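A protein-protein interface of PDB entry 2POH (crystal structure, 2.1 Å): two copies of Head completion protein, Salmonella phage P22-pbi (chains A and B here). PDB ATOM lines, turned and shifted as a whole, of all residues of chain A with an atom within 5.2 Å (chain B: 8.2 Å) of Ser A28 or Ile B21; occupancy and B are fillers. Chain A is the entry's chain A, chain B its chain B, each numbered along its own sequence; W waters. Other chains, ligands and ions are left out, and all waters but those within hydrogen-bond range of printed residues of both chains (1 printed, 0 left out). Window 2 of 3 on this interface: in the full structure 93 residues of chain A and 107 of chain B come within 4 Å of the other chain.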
ATOM      1  N   VAL A  26      20.243  34.113  16.705  1.00  0.00           N
ATOM      2  CA  VAL A  26      18.789  34.163  16.658  1.00  0.00           C
ATOM      3  C   VAL A  26      18.177  33.642  17.960  1.00  0.00           C
ATOM      4  O   VAL A  26      17.138  34.119  18.412  1.00  0.00           O
ATOM      5  CB  VAL A  26      18.222  33.320  15.499  1.00  0.00           C
ATOM      6  CG1 VAL A  26      19.343  32.631  14.733  1.00  0.00           C
ATOM      7  CG2 VAL A  26      17.227  32.302  16.036  1.00  0.00           C
ATOM      8  N   PHE A  27      18.853  32.647  18.529  1.00  0.00           N
ATOM      9  CA  PHE A  27      18.387  31.960  19.724  1.00  0.00           C
ATOM     10  C   PHE A  27      19.000  32.532  20.993  1.00  0.00           C
ATOM     11  O   PHE A  27      20.191  32.847  21.021  1.00  0.00           O
ATOM     12  CB  PHE A  27      18.727  30.469  19.655  1.00  0.00           C
ATOM     13  CG  PHE A  27      17.665  29.573  19.053  1.00  0.00           C
ATOM     14  CD1 PHE A  27      17.983  28.278  18.674  1.00  0.00           C
ATOM     15  CD2 PHE A  27      16.370  30.012  18.869  1.00  0.00           C
ATOM     16  CE1 PHE A  27      17.033  27.436  18.132  1.00  0.00           C
ATOM     17  CE2 PHE A  27      15.409  29.188  18.311  1.00  0.00           C
ATOM     18  CZ  PHE A  27      15.751  27.907  17.927  1.00  0.00           C
ATOM     19  N   SER A  28      18.196  32.647  22.046  1.00  0.00           N
ATOM     20  CA  SER A  28      18.760  33.064  23.327  1.00  0.00           C
ATOM     21  C   SER A  28      19.879  32.107  23.749  1.00  0.00           C
ATOM     22  O   SER A  28      19.976  30.989  23.237  1.00  0.00           O
ATOM     23  CB  SER A  28      17.683  33.131  24.408  1.00  0.00           C
ATOM     24  OG  SER A  28      18.197  32.781  25.683  1.00  0.00           O
ATOM     25  N   LYS A  29      20.705  32.574  24.684  1.00  0.00           N
ATOM     26  CA  LYS A  29      21.729  31.737  25.295  1.00  0.00           C
ATOM     27  C   LYS A  29      21.064  30.561  26.019  1.00  0.00           C
ATOM     28  O   LYS A  29      21.435  29.410  25.829  1.00  0.00           O
ATOM     29  CB  LYS A  29      22.603  32.542  26.250  1.00  0.00           C
ATOM     30  CG  LYS A  29      23.990  32.849  25.717  1.00  0.00           C
ATOM     31  CD  LYS A  29      23.975  33.097  24.219  1.00  0.00           C
ATOM     32  CE  LYS A  29      25.384  33.163  23.636  1.00  0.00           C
ATOM     33  NZ  LYS A  29      25.365  33.012  22.150  1.00  0.00           N
ATOM     34  N   SER A  30      20.067  30.874  26.840  1.00  0.00           N
ATOM     35  CA  SER A  30      19.285  29.875  27.550  1.00  0.00           C
ATOM     36  C   SER A  30      18.600  28.905  26.598  1.00  0.00           C
ATOM     37  O   SER A  30      18.541  27.698  26.849  1.00  0.00           O
ATOM     38  CB  SER A  30      18.241  30.560  28.442  1.00  0.00           C
ATOM     39  OG  SER A  30      18.866  31.388  29.408  1.00  0.00           O
ATOM     40  N   TYR A  31      18.066  29.397  25.466  1.00  0.00           N
ATOM     41  CA  TYR A  31      17.489  28.399  24.559  1.00  0.00           C
ATOM     42  C   TYR A  31      18.575  27.478  24.002  1.00  0.00           C
ATOM     43  O   TYR A  31      18.365  26.272  23.891  1.00  0.00           O
ATOM     44  CB  TYR A  31      16.718  29.062  23.416  1.00  0.00           C
ATOM     45  CG  TYR A  31      15.714  28.109  22.799  1.00  0.00           C
ATOM     46  CD1 TYR A  31      15.123  27.107  23.566  1.00  0.00           C
ATOM     47  CD2 TYR A  31      15.374  28.208  21.460  1.00  0.00           C
ATOM     48  CE1 TYR A  31      14.209  26.232  23.012  1.00  0.00           C
ATOM     49  CE2 TYR A  31      14.461  27.335  20.907  1.00  0.00           C
ATOM     50  CZ  TYR A  31      13.879  26.349  21.676  1.00  0.00           C
ATOM     51  OH  TYR A  31      12.969  25.493  21.090  1.00  0.00           O
ATOM     52  N   LEU A  32      19.715  28.050  23.662  1.00  0.00           N
ATOM     53  CA  LEU A  32      20.923  27.401  23.176  1.00  0.00           C
ATOM     54  C   LEU A  32      21.284  26.161  23.972  1.00  0.00           C
ATOM     55  O   LEU A  32      21.683  25.099  23.503  1.00  0.00           O
ATOM     56  CB  LEU A  32      22.050  28.435  23.258  1.00  0.00           C
ATOM     57  CG  LEU A  32      22.954  28.618  22.042  1.00  0.00           C
ATOM     58  CD1 LEU A  32      23.077  27.298  21.293  1.00  0.00           C
ATOM     59  CD2 LEU A  32      22.447  29.736  21.139  1.00  0.00           C
ATOM     60  N   THR B  15      16.082  22.406  31.872  1.00  0.00           N
ATOM     61  CA  THR B  15      15.228  23.119  32.829  1.00  0.00           C
ATOM     62  C   THR B  15      13.879  23.407  32.192  1.00  0.00           C
ATOM     63  O   THR B  15      13.801  23.507  30.966  1.00  0.00           O
ATOM     64  CB  THR B  15      15.885  24.417  33.313  1.00  0.00           C
ATOM     65  OG1 THR B  15      17.297  24.192  33.447  1.00  0.00           O
ATOM     66  CG2 THR B  15      15.354  24.793  34.688  1.00  0.00           C
ATOM     67  N   ARG B  16      12.848  23.523  33.022  1.00  0.00           N
ATOM     68  CA  ARG B  16      11.530  23.887  32.496  1.00  0.00           C
ATOM     69  C   ARG B  16      11.662  25.162  31.663  1.00  0.00           C
ATOM     70  O   ARG B  16      12.328  26.113  32.090  1.00  0.00           O
ATOM     71  CB  ARG B  16      10.519  24.044  33.627  1.00  0.00           C
ATOM     72  CG  ARG B  16       9.196  24.645  33.187  1.00  0.00           C
ATOM     73  CD  ARG B  16       8.345  23.630  32.435  1.00  0.00           C
ATOM     74  NE  ARG B  16       6.926  23.934  32.623  1.00  0.00           N
ATOM     75  CZ  ARG B  16       6.051  23.115  33.186  1.00  0.00           C
ATOM     76  NH1 ARG B  16       6.439  21.922  33.619  1.00  0.00           N
ATOM     77  NH2 ARG B  16       4.786  23.497  33.307  1.00  0.00           N
ATOM     78  N   LEU B  17      11.056  25.123  30.484  1.00  0.00           N
ATOM     79  CA  LEU B  17      11.120  26.202  29.506  1.00  0.00           C
ATOM     80  C   LEU B  17      10.365  27.434  29.993  1.00  0.00           C
ATOM     81  O   LEU B  17       9.139  27.431  30.093  1.00  0.00           O
ATOM     82  CB  LEU B  17      10.536  25.776  28.163  1.00  0.00           C
ATOM     83  CG  LEU B  17      11.451  25.671  26.947  1.00  0.00           C
ATOM     84  CD1 LEU B  17      10.661  25.119  25.763  1.00  0.00           C
ATOM     85  CD2 LEU B  17      12.087  27.008  26.599  1.00  0.00           C
ATOM     86  N   ASP B  18      11.112  28.494  30.285  1.00  0.00           N
ATOM     87  CA  ASP B  18      10.418  29.758  30.552  1.00  0.00           C
ATOM     88  C   ASP B  18      10.181  30.452  29.214  1.00  0.00           C
ATOM     89  O   ASP B  18      11.109  30.597  28.413  1.00  0.00           O
ATOM     90  CB  ASP B  18      11.210  30.618  31.524  1.00  0.00           C
ATOM     91  CG  ASP B  18      10.706  32.042  31.617  1.00  0.00           C
ATOM     92  OD1 ASP B  18      10.001  32.359  32.599  1.00  0.00           O
ATOM     93  OD2 ASP B  18      11.026  32.828  30.703  1.00  0.00           O
ATOM     94  N   ALA B  19       8.948  30.865  28.941  1.00  0.00           N
ATOM     95  CA  ALA B  19       8.700  31.445  27.619  1.00  0.00           C
ATOM     96  C   ALA B  19       9.559  32.680  27.382  1.00  0.00           C
ATOM     97  O   ALA B  19       9.831  33.045  26.235  1.00  0.00           O
ATOM     98  CB  ALA B  19       7.221  31.765  27.438  1.00  0.00           C
ATOM     99  N   SER B  20      10.014  33.350  28.440  1.00  0.00           N
ATOM    100  CA  SER B  20      10.765  34.586  28.192  1.00  0.00           C
ATOM    101  C   SER B  20      12.075  34.282  27.478  1.00  0.00           C
ATOM    102  O   SER B  20      12.605  35.116  26.746  1.00  0.00           O
ATOM    103  CB  SER B  20      10.993  35.352  29.494  1.00  0.00           C
ATOM    104  OG  SER B  20       9.759  35.826  30.017  1.00  0.00           O
ATOM    105  N   ILE B  21      12.598  33.082  27.657  1.00  0.00           N
ATOM    106  CA  ILE B  21      13.837  32.678  27.003  1.00  0.00           C
ATOM    107  C   ILE B  21      13.641  32.284  25.546  1.00  0.00           C
ATOM    108  O   ILE B  21      14.611  32.222  24.782  1.00  0.00           O
ATOM    109  CB  ILE B  21      14.504  31.524  27.786  1.00  0.00           C
ATOM    110  CG1 ILE B  21      14.002  30.134  27.416  1.00  0.00           C
ATOM    111  CG2 ILE B  21      14.366  31.785  29.277  1.00  0.00           C
ATOM    112  CD1 ILE B  21      13.974  29.158  28.579  1.00  0.00           C
ATOM    113  N   LEU B  22      12.410  32.030  25.127  1.00  0.00           N
ATOM    114  CA  LEU B  22      12.133  31.692  23.731  1.00  0.00           C
ATOM    115  C   LEU B  22      12.249  32.942  22.861  1.00  0.00           C
ATOM    116  O   LEU B  22      12.156  34.029  23.428  1.00  0.00           O
ATOM    117  CB  LEU B  22      10.757  31.027  23.610  1.00  0.00           C
ATOM    118  CG  LEU B  22      10.731  29.536  23.979  1.00  0.00           C
ATOM    119  CD1 LEU B  22       9.376  28.911  23.681  1.00  0.00           C
ATOM    120  CD2 LEU B  22      11.840  28.793  23.243  1.00  0.00           C
ATOM    121  N   PRO B  23      12.455  32.814  21.559  1.00  0.00           N
ATOM    122  CA  PRO B  23      12.589  33.959  20.650  1.00  0.00           C
ATOM    123  C   PRO B  23      11.269  34.308  19.962  1.00  0.00           C
ATOM    124  O   PRO B  23      11.064  33.944  18.806  1.00  0.00           O
ATOM    125  CB  PRO B  23      13.573  33.430  19.603  1.00  0.00           C
ATOM    126  CG  PRO B  23      13.331  31.957  19.566  1.00  0.00           C
ATOM    127  CD  PRO B  23      12.589  31.557  20.802  1.00  0.00           C
ATOM    128  N   ARG B  24      10.405  34.993  20.692  1.00  0.00           N
ATOM    129  CA  ARG B  24       9.014  35.190  20.318  1.00  0.00           C
ATOM    130  C   ARG B  24       8.841  36.164  19.171  1.00  0.00           C
ATOM    131  O   ARG B  24       7.790  36.238  18.519  1.00  0.00           O
ATOM    132  CB  ARG B  24       8.227  35.654  21.550  1.00  0.00           C
ATOM    133  CG  ARG B  24       8.748  36.961  22.137  1.00  0.00           C
ATOM    134  CD  ARG B  24       7.593  37.912  22.412  1.00  0.00           C
ATOM    135  NE  ARG B  24       8.029  39.266  22.734  1.00  0.00           N
ATOM    136  CZ  ARG B  24       7.653  39.882  23.852  1.00  0.00           C
ATOM    137  NH1 ARG B  24       6.860  39.236  24.698  1.00  0.00           N
ATOM    138  NH2 ARG B  24       8.064  41.113  24.115  1.00  0.00           N
ATOM    139  N   PHE B  27       9.347  33.202  16.626  1.00  0.00           N
ATOM    140  CA  PHE B  27       8.586  31.964  16.743  1.00  0.00           C
ATOM    141  C   PHE B  27       7.089  32.202  16.602  1.00  0.00           C
ATOM    142  O   PHE B  27       6.494  32.974  17.353  1.00  0.00           O
ATOM    143  CB  PHE B  27       8.883  31.294  18.087  1.00  0.00           C
ATOM    144  CG  PHE B  27      10.055  30.325  18.011  1.00  0.00           C
ATOM    145  CD1 PHE B  27      11.121  30.585  17.168  1.00  0.00           C
ATOM    146  CD2 PHE B  27      10.072  29.175  18.779  1.00  0.00           C
ATOM    147  CE1 PHE B  27      12.188  29.714  17.090  1.00  0.00           C
ATOM    148  CE2 PHE B  27      11.136  28.297  18.703  1.00  0.00           C
ATOM    149  CZ  PHE B  27      12.194  28.566  17.856  1.00  0.00           C
ATOM    150  N   LEU B  32       5.321  27.805  19.299  1.00  0.00           N
ATOM    151  CA  LEU B  32       5.656  28.228  20.657  1.00  0.00           C
ATOM    152  C   LEU B  32       5.021  27.273  21.665  1.00  0.00           C
ATOM    153  O   LEU B  32       5.610  26.878  22.669  1.00  0.00           O
ATOM    154  CB  LEU B  32       5.208  29.667  20.904  1.00  0.00           C
ATOM    155  CG  LEU B  32       6.275  30.664  21.350  1.00  0.00           C
ATOM    156  CD1 LEU B  32       7.670  30.158  21.003  1.00  0.00           C
ATOM    157  CD2 LEU B  32       6.062  32.039  20.735  1.00  0.00           C
ATOM    158  N   VAL B  35       6.582  23.633  21.075  1.00  0.00           N
ATOM    159  CA  VAL B  35       7.853  23.678  21.781  1.00  0.00           C
ATOM    160  C   VAL B  35       7.653  23.548  23.281  1.00  0.00           C
ATOM    161  O   VAL B  35       8.421  22.892  23.990  1.00  0.00           O
ATOM    162  CB  VAL B  35       8.591  24.991  21.428  1.00  0.00           C
ATOM    163  CG1 VAL B  35       9.524  25.436  22.541  1.00  0.00           C
ATOM    164  CG2 VAL B  35       9.355  24.837  20.123  1.00  0.00           C
ATOM    165  N   ILE B  36       6.592  24.157  23.804  1.00  0.00           N
ATOM    166  CA  ILE B  36       6.317  24.053  25.235  1.00  0.00           C
ATOM    167  C   ILE B  36       5.768  22.660  25.561  1.00  0.00           C
ATOM    168  O   ILE B  36       6.078  22.113  26.611  1.00  0.00           O
ATOM    169  CB  ILE B  36       5.298  25.075  25.766  1.00  0.00           C
ATOM    170  CG1 ILE B  36       5.597  26.534  25.443  1.00  0.00           C
ATOM    171  CG2 ILE B  36       5.122  24.926  27.274  1.00  0.00           C
ATOM    172  CD1 ILE B  36       7.039  26.824  25.095  1.00  0.00           C
HETATM  173  O   HOH W   1      15.198  32.964  22.263  1.00  0.00           O
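N of Tyr A31 sits at hydrogen-bond distance from OG of Ser A28 (3.4 Å).
OD2 of Asp B18 sits at hydrogen-bond distance from N of Ile B21.
The side-chain hydroxyl of Ser A28 lies within hydrogen-bond range of the backbone NH of Ser A30 (2.9 Å).
Among the printed residues, pairs that only touch across the chains: Ser A28 with Ile B21, Phe A27 with Phe B27, Tyr A31 with Leu B22, Phe A27 with Pro B23, Tyr A31 with Val B35, Val A26 with Pro B23, Ser A30 with Ile B21 and Tyr A31 with Phe B27.
Of the printed residues of chain B, Val A26 touches Pro B23.
Of the printed residues of chain B, Phe A27 touches Pro B23 and Phe B27.
Of chain B, only Ile B21 (3.2 Å) comes within 4 Å of Ser A28.
Of the printed residues of chain B, Ser A30 touches Ile B21 (3.9 Å).
Asp B18 touches none of the printed residues of chain A.
Of chain A, only Ser A28 and Ser A30 come within 4 Å of Ile B21.
Of the printed residues of chain A, Pro B23 touches Val A26 and Phe A27.
The nearest residue of chain A that does not touch Ile B21 is Tyr A31 (4.04 Å).
Of the 7 printed residues of chain A, 5 touch a printed residue of chain B.
Printed residues of chain A that touch a printed residue of chain B: Val A26, Phe A27, Ser A28, Ser A30 and Tyr A31.
Phe B27 touches its own counterpart, Phe A27.
Water W1 lies within hydrogen-bond range of O of Ile B21 (2.7 Å), N of Ser A28 (3.0 Å) and O of Leu B22 (3.4 Å).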
